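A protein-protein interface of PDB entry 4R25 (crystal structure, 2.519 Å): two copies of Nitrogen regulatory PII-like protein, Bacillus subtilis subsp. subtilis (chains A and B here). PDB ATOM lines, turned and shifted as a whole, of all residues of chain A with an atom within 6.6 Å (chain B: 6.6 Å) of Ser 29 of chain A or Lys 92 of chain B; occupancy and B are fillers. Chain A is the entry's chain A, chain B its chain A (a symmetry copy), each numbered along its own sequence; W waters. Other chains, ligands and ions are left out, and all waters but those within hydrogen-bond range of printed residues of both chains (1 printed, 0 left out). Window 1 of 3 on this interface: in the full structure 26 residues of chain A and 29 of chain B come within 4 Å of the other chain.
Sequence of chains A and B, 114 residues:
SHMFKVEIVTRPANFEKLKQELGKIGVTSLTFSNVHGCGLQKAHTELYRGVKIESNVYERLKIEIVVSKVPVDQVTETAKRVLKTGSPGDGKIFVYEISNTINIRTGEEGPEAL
The backbone NH (N) of Leu 40 of chain B is in hydrogen-bond range of the backbone carbonyl oxygen (O) of Thr 28 of chain A (2.8 Å).
The side-chain hydroxyl (OG) of Ser 29 of chain A sits at hydrogen-bond distance from the side-chain amino group (NZ) of Lys 92 of chain B.
The backbone carbonyl oxygen (O) of Leu 30 of chain A sits at hydrogen-bond distance from the backbone NH (N) of Cys 38 of chain B, 2.9 Å away.
O of Ile 102 of chain A sits at hydrogen-bond distance from N of Ile 93 of chain B (2.9 Å).
The backbone NH of Ile 104 of chain A lies within hydrogen-bond range of the backbone carbonyl oxygen of Gly 91 of chain B, at 3.1 Å.
O of Thr 31 of chain A lies within hydrogen-bond range of N of Glu 64 of chain A.
The side-chain amide nitrogen (ND2) of Asn 103 of chain A sits at hydrogen-bond distance from the backbone carbonyl oxygen (O) of Ala 113 of chain A (3.0 Å).
N of Phe 94 of chain B sits at hydrogen-bond distance from O of Glu 7 of chain B (2.8 Å).
The backbone NH of Val 9 of chain B lies within hydrogen-bond range of the backbone carbonyl oxygen of Lys 92 of chain B.
OG1 of Thr 10 of chain B sits at hydrogen-bond distance from O of Asp 90 of chain B, 3.0 Å away.
O of Gly 37 of chain B is in hydrogen-bond range of N of Tyr 58 of chain B.
O of Cys 38 of chain B touches CA of Ser 29 of chain A, 3.1 Å away.
CG1 of Val 9 of chain B touches CG2 of Thr 31 of chain A (3.96 Å).
CE1 of Phe 94 of chain B touches CG2 of Val 66 of chain A, 3.4 Å away.
Thr 101 of chain A touches Ile 93 of chain B.
Ile 102 of chain A touches Lys 92 of chain B.
CD1 of Ile 104 of chain A touches O of Asp 90 of chain B, at 3.3 Å.
Ile 104 of chain A touches Lys 92 of chain B (CD1 to N, 3.8 Å).
Ile 93 of chain B touches Ile 104 of chain A.
CE of Lys 92 of chain B touches O of Ala 113 of chain A (3.9 Å).
Lys 92 of chain B touches Leu 114 of chain A (CE to OXT, 3.8 Å).
Printed residues of chain B within 4 Å of Thr 28 of chain A: Gly 39 (3.5 Å) and Leu 40 (2.8 Å).
Ser 29 of chain A touches two residues of chain B.
Glu 64 of chain A touches none of the printed residues of chain B.
Of the printed residues of chain B, Ile 102 of chain A touches Lys 92 and Ile 93.
Of the printed residues of chain A, Val 9 of chain B touches Thr 31 (3.96 Å).
Of the printed residues of chain A, Cys 38 of chain B touches Ser 29 and Leu 30.
Of the printed residues of chain A, Asp 90 of chain B touches Ile 104 (3.3 Å).
Of chain A, only Ser 29 (3.5 Å), Ile 102 (3.2 Å), Ile 104 (3.8 Å), Ala 113 (3.9 Å) and Leu 114 (3.8 Å) come within 4 Å of Lys 92 of chain B.
The nearest residue of chain B that does not touch Ser 29 of chain A is Tyr 58 of chain B (4.3 Å).
The nearest printed residue of chain A that does not touch Lys 92 of chain B is Thr 101 of chain A (4.4 Å).
The nearest printed residue of chain B that does not touch Val 27 of chain A is Gly 39 of chain B (6.3 Å).
Printed residues of chain A that touch a printed residue of chain B: Val 27, Thr 28, Ser 29, Leu 30, Thr 31, Val 66, Thr 101, Ile 102, Ile 104, Ala 113 and Leu 114.
Of the 14 printed residues of chain B, 10 touch a printed residue of chain A.
No position is printed for both chains.
Of the 19 pairs that touch across the chains among the printed residues, none has its exchanged pair printed and touching as well.
Water W1 lies within hydrogen-bond range of the side-chain carboxylate (OE1) of Glu 64 of chain A (2.9 Å) and the side-chain carboxylate (OE1) of Glu 7 of chain B (2.9 Å).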
ATOM      1  N   GLY A  26     -36.333  -4.075  25.615  1.00  0.00           N
ATOM      2  CA  GLY A  26     -35.023  -4.705  25.609  1.00  0.00           C
ATOM      3  C   GLY A  26     -33.791  -3.829  25.786  1.00  0.00           C
ATOM      4  O   GLY A  26     -32.702  -4.358  26.001  1.00  0.00           O
ATOM      5  N   VAL A  27     -33.937  -2.507  25.697  1.00  0.00           N
ATOM      6  CA  VAL A  27     -32.784  -1.624  25.863  1.00  0.00           C
ATOM      7  C   VAL A  27     -32.272  -1.631  27.300  1.00  0.00           C
ATOM      8  O   VAL A  27     -33.041  -1.414  28.239  1.00  0.00           O
ATOM      9  CB  VAL A  27     -33.088  -0.175  25.466  1.00  0.00           C
ATOM     10  CG1 VAL A  27     -31.849   0.677  25.660  1.00  0.00           C
ATOM     11  CG2 VAL A  27     -33.581  -0.106  24.028  1.00  0.00           C
ATOM     12  N   THR A  28     -30.972  -1.868  27.466  1.00  0.00           N
ATOM     13  CA  THR A  28     -30.371  -1.928  28.798  1.00  0.00           C
ATOM     14  C   THR A  28     -29.417  -0.770  29.111  1.00  0.00           C
ATOM     15  O   THR A  28     -28.974  -0.618  30.245  1.00  0.00           O
ATOM     16  CB  THR A  28     -29.645  -3.261  29.031  1.00  0.00           C
ATOM     17  OG1 THR A  28     -28.471  -3.319  28.213  1.00  0.00           O
ATOM     18  CG2 THR A  28     -30.553  -4.427  28.676  1.00  0.00           C
ATOM     19  N   SER A  29     -29.095   0.045  28.110  1.00  0.00           N
ATOM     20  CA  SER A  29     -28.332   1.272  28.355  1.00  0.00           C
ATOM     21  C   SER A  29     -28.459   2.308  27.228  1.00  0.00           C
ATOM     22  O   SER A  29     -28.759   1.981  26.078  1.00  0.00           O
ATOM     23  CB  SER A  29     -26.854   0.970  28.649  1.00  0.00           C
ATOM     24  OG  SER A  29     -26.147   0.576  27.487  1.00  0.00           O
ATOM     25  N   LEU A  30     -28.228   3.564  27.579  1.00  0.00           N
ATOM     26  CA  LEU A  30     -28.262   4.641  26.609  1.00  0.00           C
ATOM     27  C   LEU A  30     -27.476   5.836  27.146  1.00  0.00           C
ATOM     28  O   LEU A  30     -27.184   5.907  28.338  1.00  0.00           O
ATOM     29  CB  LEU A  30     -29.713   5.020  26.304  1.00  0.00           C
ATOM     30  CG  LEU A  30     -30.557   5.470  27.496  1.00  0.00           C
ATOM     31  CD1 LEU A  30     -30.268   6.916  27.841  1.00  0.00           C
ATOM     32  CD2 LEU A  30     -32.047   5.266  27.240  1.00  0.00           C
ATOM     33  N   THR A  31     -27.123   6.769  26.268  1.00  0.00           N
ATOM     34  CA  THR A  31     -26.452   7.990  26.705  1.00  0.00           C
ATOM     35  C   THR A  31     -27.301   9.209  26.376  1.00  0.00           C
ATOM     36  O   THR A  31     -28.109   9.188  25.453  1.00  0.00           O
ATOM     37  CB  THR A  31     -25.075   8.147  26.051  1.00  0.00           C
ATOM     38  OG1 THR A  31     -25.211   8.027  24.633  1.00  0.00           O
ATOM     39  CG2 THR A  31     -24.114   7.070  26.556  1.00  0.00           C
ATOM     40  N   GLU A  64     -28.847   8.846  22.851  1.00  0.00           N
ATOM     41  CA  GLU A  64     -28.257   7.851  21.969  1.00  0.00           C
ATOM     42  C   GLU A  64     -28.444   6.406  22.465  1.00  0.00           C
ATOM     43  O   GLU A  64     -28.187   6.074  23.622  1.00  0.00           O
ATOM     44  CB  GLU A  64     -26.788   8.169  21.735  1.00  0.00           C
ATOM     45  CG  GLU A  64     -26.584   9.484  21.000  1.00  0.00           C
ATOM     46  CD  GLU A  64     -25.122   9.797  20.747  1.00  0.00           C
ATOM     47  OE1 GLU A  64     -24.252   9.295  21.492  1.00  0.00           O
ATOM     48  OE2 GLU A  64     -24.842  10.545  19.793  1.00  0.00           O
ATOM     49  N   ILE A  65     -28.906   5.558  21.561  1.00  0.00           N
ATOM     50  CA  ILE A  65     -29.162   4.171  21.856  1.00  0.00           C
ATOM     51  C   ILE A  65     -28.517   3.351  20.756  1.00  0.00           C
ATOM     52  O   ILE A  65     -28.709   3.629  19.577  1.00  0.00           O
ATOM     53  CB  ILE A  65     -30.673   3.900  21.883  1.00  0.00           C
ATOM     54  CG1 ILE A  65     -31.375   4.973  22.716  1.00  0.00           C
ATOM     55  CG2 ILE A  65     -30.966   2.516  22.431  1.00  0.00           C
ATOM     56  CD1 ILE A  65     -32.850   5.104  22.427  1.00  0.00           C
ATOM     57  N   VAL A  66     -27.713   2.368  21.137  1.00  0.00           N
ATOM     58  CA  VAL A  66     -27.161   1.439  20.166  1.00  0.00           C
ATOM     59  C   VAL A  66     -27.938   0.142  20.274  1.00  0.00           C
ATOM     60  O   VAL A  66     -28.285  -0.281  21.368  1.00  0.00           O
ATOM     61  CB  VAL A  66     -25.670   1.183  20.418  1.00  0.00           C
ATOM     62  CG1 VAL A  66     -25.116   0.181  19.404  1.00  0.00           C
ATOM     63  CG2 VAL A  66     -24.905   2.495  20.360  1.00  0.00           C
ATOM     64  N   THR A 101     -18.863  -2.552  17.287  1.00  0.00           N
ATOM     65  CA  THR A 101     -18.933  -2.180  18.688  1.00  0.00           C
ATOM     66  C   THR A 101     -17.982  -3.058  19.485  1.00  0.00           C
ATOM     67  O   THR A 101     -17.779  -4.222  19.168  1.00  0.00           O
ATOM     68  CB  THR A 101     -20.342  -2.370  19.253  1.00  0.00           C
ATOM     69  OG1 THR A 101     -21.282  -1.688  18.419  1.00  0.00           O
ATOM     70  CG2 THR A 101     -20.429  -1.824  20.678  1.00  0.00           C
ATOM     71  N   ILE A 102     -17.403  -2.487  20.526  1.00  0.00           N
ATOM     72  CA  ILE A 102     -16.449  -3.204  21.338  1.00  0.00           C
ATOM     73  C   ILE A 102     -16.754  -2.925  22.788  1.00  0.00           C
ATOM     74  O   ILE A 102     -16.770  -1.775  23.214  1.00  0.00           O
ATOM     75  CB  ILE A 102     -15.013  -2.772  21.030  1.00  0.00           C
ATOM     76  CG1 ILE A 102     -14.652  -3.158  19.598  1.00  0.00           C
ATOM     77  CG2 ILE A 102     -14.039  -3.391  22.015  1.00  0.00           C
ATOM     78  CD1 ILE A 102     -13.288  -2.694  19.170  1.00  0.00           C
ATOM     79  N   ASN A 103     -17.028  -3.987  23.534  1.00  0.00           N
ATOM     80  CA  ASN A 103     -17.186  -3.873  24.965  1.00  0.00           C
ATOM     81  C   ASN A 103     -15.812  -3.856  25.592  1.00  0.00           C
ATOM     82  O   ASN A 103     -15.025  -4.779  25.407  1.00  0.00           O
ATOM     83  CB  ASN A 103     -17.989  -5.039  25.521  1.00  0.00           C
ATOM     84  CG  ASN A 103     -18.395  -4.818  26.950  1.00  0.00           C
ATOM     85  OD1 ASN A 103     -17.569  -4.486  27.805  1.00  0.00           O
ATOM     86  ND2 ASN A 103     -19.684  -4.958  27.218  1.00  0.00           N
ATOM     87  N   ILE A 104     -15.522  -2.802  26.336  1.00  0.00           N
ATOM     88  CA  ILE A 104     -14.173  -2.598  26.829  1.00  0.00           C
ATOM     89  C   ILE A 104     -13.795  -3.582  27.931  1.00  0.00           C
ATOM     90  O   ILE A 104     -12.676  -4.088  27.952  1.00  0.00           O
ATOM     91  CB  ILE A 104     -13.960  -1.144  27.269  1.00  0.00           C
ATOM     92  CG1 ILE A 104     -13.956  -0.236  26.036  1.00  0.00           C
ATOM     93  CG2 ILE A 104     -12.659  -1.006  28.036  1.00  0.00           C
ATOM     94  CD1 ILE A 104     -13.950   1.234  26.356  1.00  0.00           C
ATOM     95  N   ALA A 113     -21.140  -7.428  22.067  1.00  0.00           N
ATOM     96  CA  ALA A 113     -20.528  -6.409  22.908  1.00  0.00           C
ATOM     97  C   ALA A 113     -21.598  -5.582  23.622  1.00  0.00           C
ATOM     98  O   ALA A 113     -21.362  -5.043  24.702  1.00  0.00           O
ATOM     99  CB  ALA A 113     -19.618  -5.513  22.081  1.00  0.00           C
ATOM    100  N   LEU A 114     -22.780  -5.508  23.015  1.00  0.00           N
ATOM    101  CA  LEU A 114     -23.870  -4.689  23.535  1.00  0.00           C
ATOM    102  C   LEU A 114     -24.446  -5.241  24.839  1.00  0.00           C
ATOM    103  O   LEU A 114     -24.808  -6.416  24.955  1.00  0.00           O
ATOM    104  CB  LEU A 114     -24.964  -4.499  22.475  1.00  0.00           C
ATOM    105  CG  LEU A 114     -24.494  -3.771  21.221  1.00  0.00           C
ATOM    106  CD1 LEU A 114     -25.631  -3.506  20.246  1.00  0.00           C
ATOM    107  CD2 LEU A 114     -23.861  -2.477  21.645  1.00  0.00           C
ATOM    108  OXT LEU A 114     -24.547  -4.498  25.823  1.00  0.00           O
ATOM    109  N   GLU B   7     -15.627   6.251  18.374  1.00  0.00           N
ATOM    110  CA  GLU B   7     -16.326   6.868  19.486  1.00  0.00           C
ATOM    111  C   GLU B   7     -16.173   6.028  20.754  1.00  0.00           C
ATOM    112  O   GLU B   7     -16.719   4.929  20.852  1.00  0.00           O
ATOM    113  CB  GLU B   7     -17.794   7.011  19.125  1.00  0.00           C
ATOM    114  CG  GLU B   7     -18.592   7.917  20.013  1.00  0.00           C
ATOM    115  CD  GLU B   7     -19.912   8.292  19.365  1.00  0.00           C
ATOM    116  OE1 GLU B   7     -20.970   7.762  19.773  1.00  0.00           O
ATOM    117  OE2 GLU B   7     -19.885   9.114  18.426  1.00  0.00           O
ATOM    118  N   ILE B   8     -15.418   6.542  21.718  1.00  0.00           N
ATOM    119  CA  ILE B   8     -15.240   5.853  22.980  1.00  0.00           C
ATOM    120  C   ILE B   8     -16.127   6.479  24.047  1.00  0.00           C
ATOM    121  O   ILE B   8     -16.027   7.673  24.323  1.00  0.00           O
ATOM    122  CB  ILE B   8     -13.773   5.911  23.448  1.00  0.00           C
ATOM    123  CG1 ILE B   8     -12.831   5.509  22.312  1.00  0.00           C
ATOM    124  CG2 ILE B   8     -13.571   5.016  24.656  1.00  0.00           C
ATOM    125  CD1 ILE B   8     -11.362   5.763  22.612  1.00  0.00           C
ATOM    126  N   VAL B   9     -17.002   5.680  24.642  1.00  0.00           N
ATOM    127  CA  VAL B   9     -17.864   6.172  25.710  1.00  0.00           C
ATOM    128  C   VAL B   9     -17.544   5.447  27.017  1.00  0.00           C
ATOM    129  O   VAL B   9     -17.865   4.275  27.185  1.00  0.00           O
ATOM    130  CB  VAL B   9     -19.352   6.000  25.359  1.00  0.00           C
ATOM    131  CG1 VAL B   9     -20.220   6.337  26.551  1.00  0.00           C
ATOM    132  CG2 VAL B   9     -19.713   6.867  24.164  1.00  0.00           C
ATOM    133  N   THR B  10     -16.914   6.154  27.947  1.00  0.00           N
ATOM    134  CA  THR B  10     -16.289   5.477  29.067  1.00  0.00           C
ATOM    135  C   THR B  10     -16.275   6.262  30.386  1.00  0.00           C
ATOM    136  O   THR B  10     -16.855   7.341  30.497  1.00  0.00           O
ATOM    137  CB  THR B  10     -14.869   5.003  28.664  1.00  0.00           C
ATOM    138  OG1 THR B  10     -14.210   4.387  29.775  1.00  0.00           O
ATOM    139  CG2 THR B  10     -14.034   6.166  28.144  1.00  0.00           C
ATOM    140  N   GLY B  37     -24.618   8.436  31.229  1.00  0.00           N
ATOM    141  CA  GLY B  37     -25.006   7.086  30.899  1.00  0.00           C
ATOM    142  C   GLY B  37     -26.188   6.697  31.763  1.00  0.00           C
ATOM    143  O   GLY B  37     -26.344   7.157  32.892  1.00  0.00           O
ATOM    144  N   CYS B  38     -27.037   5.847  31.219  1.00  0.00           N
ATOM    145  CA  CYS B  38     -28.200   5.386  31.944  1.00  0.00           C
ATOM    146  C   CYS B  38     -28.307   3.896  31.732  1.00  0.00           C
ATOM    147  O   CYS B  38     -28.400   3.437  30.594  1.00  0.00           O
ATOM    148  CB  CYS B  38     -29.459   6.085  31.428  1.00  0.00           C
ATOM    149  SG  CYS B  38     -30.944   5.686  32.343  1.00  0.00           S
ATOM    150  N   GLY B  39     -28.264   3.142  32.827  1.00  0.00           N
ATOM    151  CA  GLY B  39     -28.518   1.715  32.780  1.00  0.00           C
ATOM    152  C   GLY B  39     -29.998   1.441  32.977  1.00  0.00           C
ATOM    153  O   GLY B  39     -30.664   2.123  33.747  1.00  0.00           O
ATOM    154  N   LEU B  40     -30.518   0.451  32.265  1.00  0.00           N
ATOM    155  CA  LEU B  40     -31.916   0.075  32.382  1.00  0.00           C
ATOM    156  C   LEU B  40     -32.033  -1.428  32.658  1.00  0.00           C
ATOM    157  O   LEU B  40     -31.429  -2.248  31.968  1.00  0.00           O
ATOM    158  CB  LEU B  40     -32.686   0.446  31.108  1.00  0.00           C
ATOM    159  CG  LEU B  40     -32.688   1.900  30.623  1.00  0.00           C
ATOM    160  CD1 LEU B  40     -33.599   2.051  29.428  1.00  0.00           C
ATOM    161  CD2 LEU B  40     -33.113   2.862  31.706  1.00  0.00           C
ATOM    162  N   TYR B  58     -25.131   7.608  35.467  1.00  0.00           N
ATOM    163  CA  TYR B  58     -23.732   7.798  35.837  1.00  0.00           C
ATOM    164  C   TYR B  58     -23.030   8.798  34.916  1.00  0.00           C
ATOM    165  O   TYR B  58     -23.635   9.338  33.987  1.00  0.00           O
ATOM    166  CB  TYR B  58     -22.992   6.455  35.865  1.00  0.00           C
ATOM    167  CG  TYR B  58     -23.396   5.524  34.753  1.00  0.00           C
ATOM    168  CD1 TYR B  58     -24.548   4.752  34.854  1.00  0.00           C
ATOM    169  CD2 TYR B  58     -22.630   5.413  33.596  1.00  0.00           C
ATOM    170  CE1 TYR B  58     -24.937   3.901  33.832  1.00  0.00           C
ATOM    171  CE2 TYR B  58     -23.006   4.559  32.568  1.00  0.00           C
ATOM    172  CZ  TYR B  58     -24.163   3.807  32.691  1.00  0.00           C
ATOM    173  OH  TYR B  58     -24.547   2.962  31.675  1.00  0.00           O
ATOM    174  N   ASP B  90     -16.659   0.122  32.324  1.00  0.00           N
ATOM    175  CA  ASP B  90     -15.478   0.293  31.489  1.00  0.00           C
ATOM    176  C   ASP B  90     -15.841   0.959  30.165  1.00  0.00           C
ATOM    177  O   ASP B  90     -14.990   1.533  29.493  1.00  0.00           O
ATOM    178  CB  ASP B  90     -14.808  -1.059  31.234  1.00  0.00           C
ATOM    179  CG  ASP B  90     -13.754  -1.399  32.277  1.00  0.00           C
ATOM    180  OD1 ASP B  90     -13.604  -0.631  33.251  1.00  0.00           O
ATOM    181  OD2 ASP B  90     -13.077  -2.437  32.124  1.00  0.00           O
ATOM    182  N   GLY B  91     -17.110   0.862  29.789  1.00  0.00           N
ATOM    183  CA  GLY B  91     -17.602   1.535  28.608  1.00  0.00           C
ATOM    184  C   GLY B  91     -17.502   0.741  27.325  1.00  0.00           C
ATOM    185  O   GLY B  91     -17.183  -0.441  27.329  1.00  0.00           O
ATOM    186  N   LYS B  92     -17.779   1.413  26.215  1.00  0.00           N
ATOM    187  CA  LYS B  92     -17.825   0.774  24.907  1.00  0.00           C
ATOM    188  C   LYS B  92     -17.128   1.630  23.853  1.00  0.00           C
ATOM    189  O   LYS B  92     -16.726   2.763  24.114  1.00  0.00           O
ATOM    190  CB  LYS B  92     -19.275   0.501  24.492  1.00  0.00           C
ATOM    191  CG  LYS B  92     -20.111  -0.204  25.559  1.00  0.00           C
ATOM    192  CD  LYS B  92     -21.283  -0.962  24.946  1.00  0.00           C
ATOM    193  CE  LYS B  92     -22.225  -1.502  26.015  1.00  0.00           C
ATOM    194  NZ  LYS B  92     -22.881  -0.400  26.778  1.00  0.00           N
ATOM    195  N   ILE B  93     -16.981   1.072  22.659  1.00  0.00           N
ATOM    196  CA  ILE B  93     -16.322   1.769  21.577  1.00  0.00           C
ATOM    197  C   ILE B  93     -17.116   1.518  20.320  1.00  0.00           C
ATOM    198  O   ILE B  93     -17.358   0.374  19.969  1.00  0.00           O
ATOM    199  CB  ILE B  93     -14.904   1.229  21.340  1.00  0.00           C
ATOM    200  CG1 ILE B  93     -14.045   1.399  22.591  1.00  0.00           C
ATOM    201  CG2 ILE B  93     -14.255   1.917  20.134  1.00  0.00           C
ATOM    202  CD1 ILE B  93     -12.697   0.749  22.467  1.00  0.00           C
ATOM    203  N   PHE B  94     -17.502   2.586  19.631  1.00  0.00           N
ATOM    204  CA  PHE B  94     -18.279   2.448  18.412  1.00  0.00           C
ATOM    205  C   PHE B  94     -17.517   2.959  17.196  1.00  0.00           C
ATOM    206  O   PHE B  94     -16.869   4.002  17.248  1.00  0.00           O
ATOM    207  CB  PHE B  94     -19.621   3.169  18.558  1.00  0.00           C
ATOM    208  CG  PHE B  94     -20.344   2.839  19.835  1.00  0.00           C
ATOM    209  CD1 PHE B  94     -21.099   1.684  19.942  1.00  0.00           C
ATOM    210  CD2 PHE B  94     -20.259   3.677  20.930  1.00  0.00           C
ATOM    211  CE1 PHE B  94     -21.769   1.376  21.119  1.00  0.00           C
ATOM    212  CE2 PHE B  94     -20.921   3.374  22.108  1.00  0.00           C
ATOM    213  CZ  PHE B  94     -21.680   2.225  22.202  1.00  0.00           C
HETATM  214  O   HOH W   1     -22.874   6.796  21.781  1.00  0.00           O
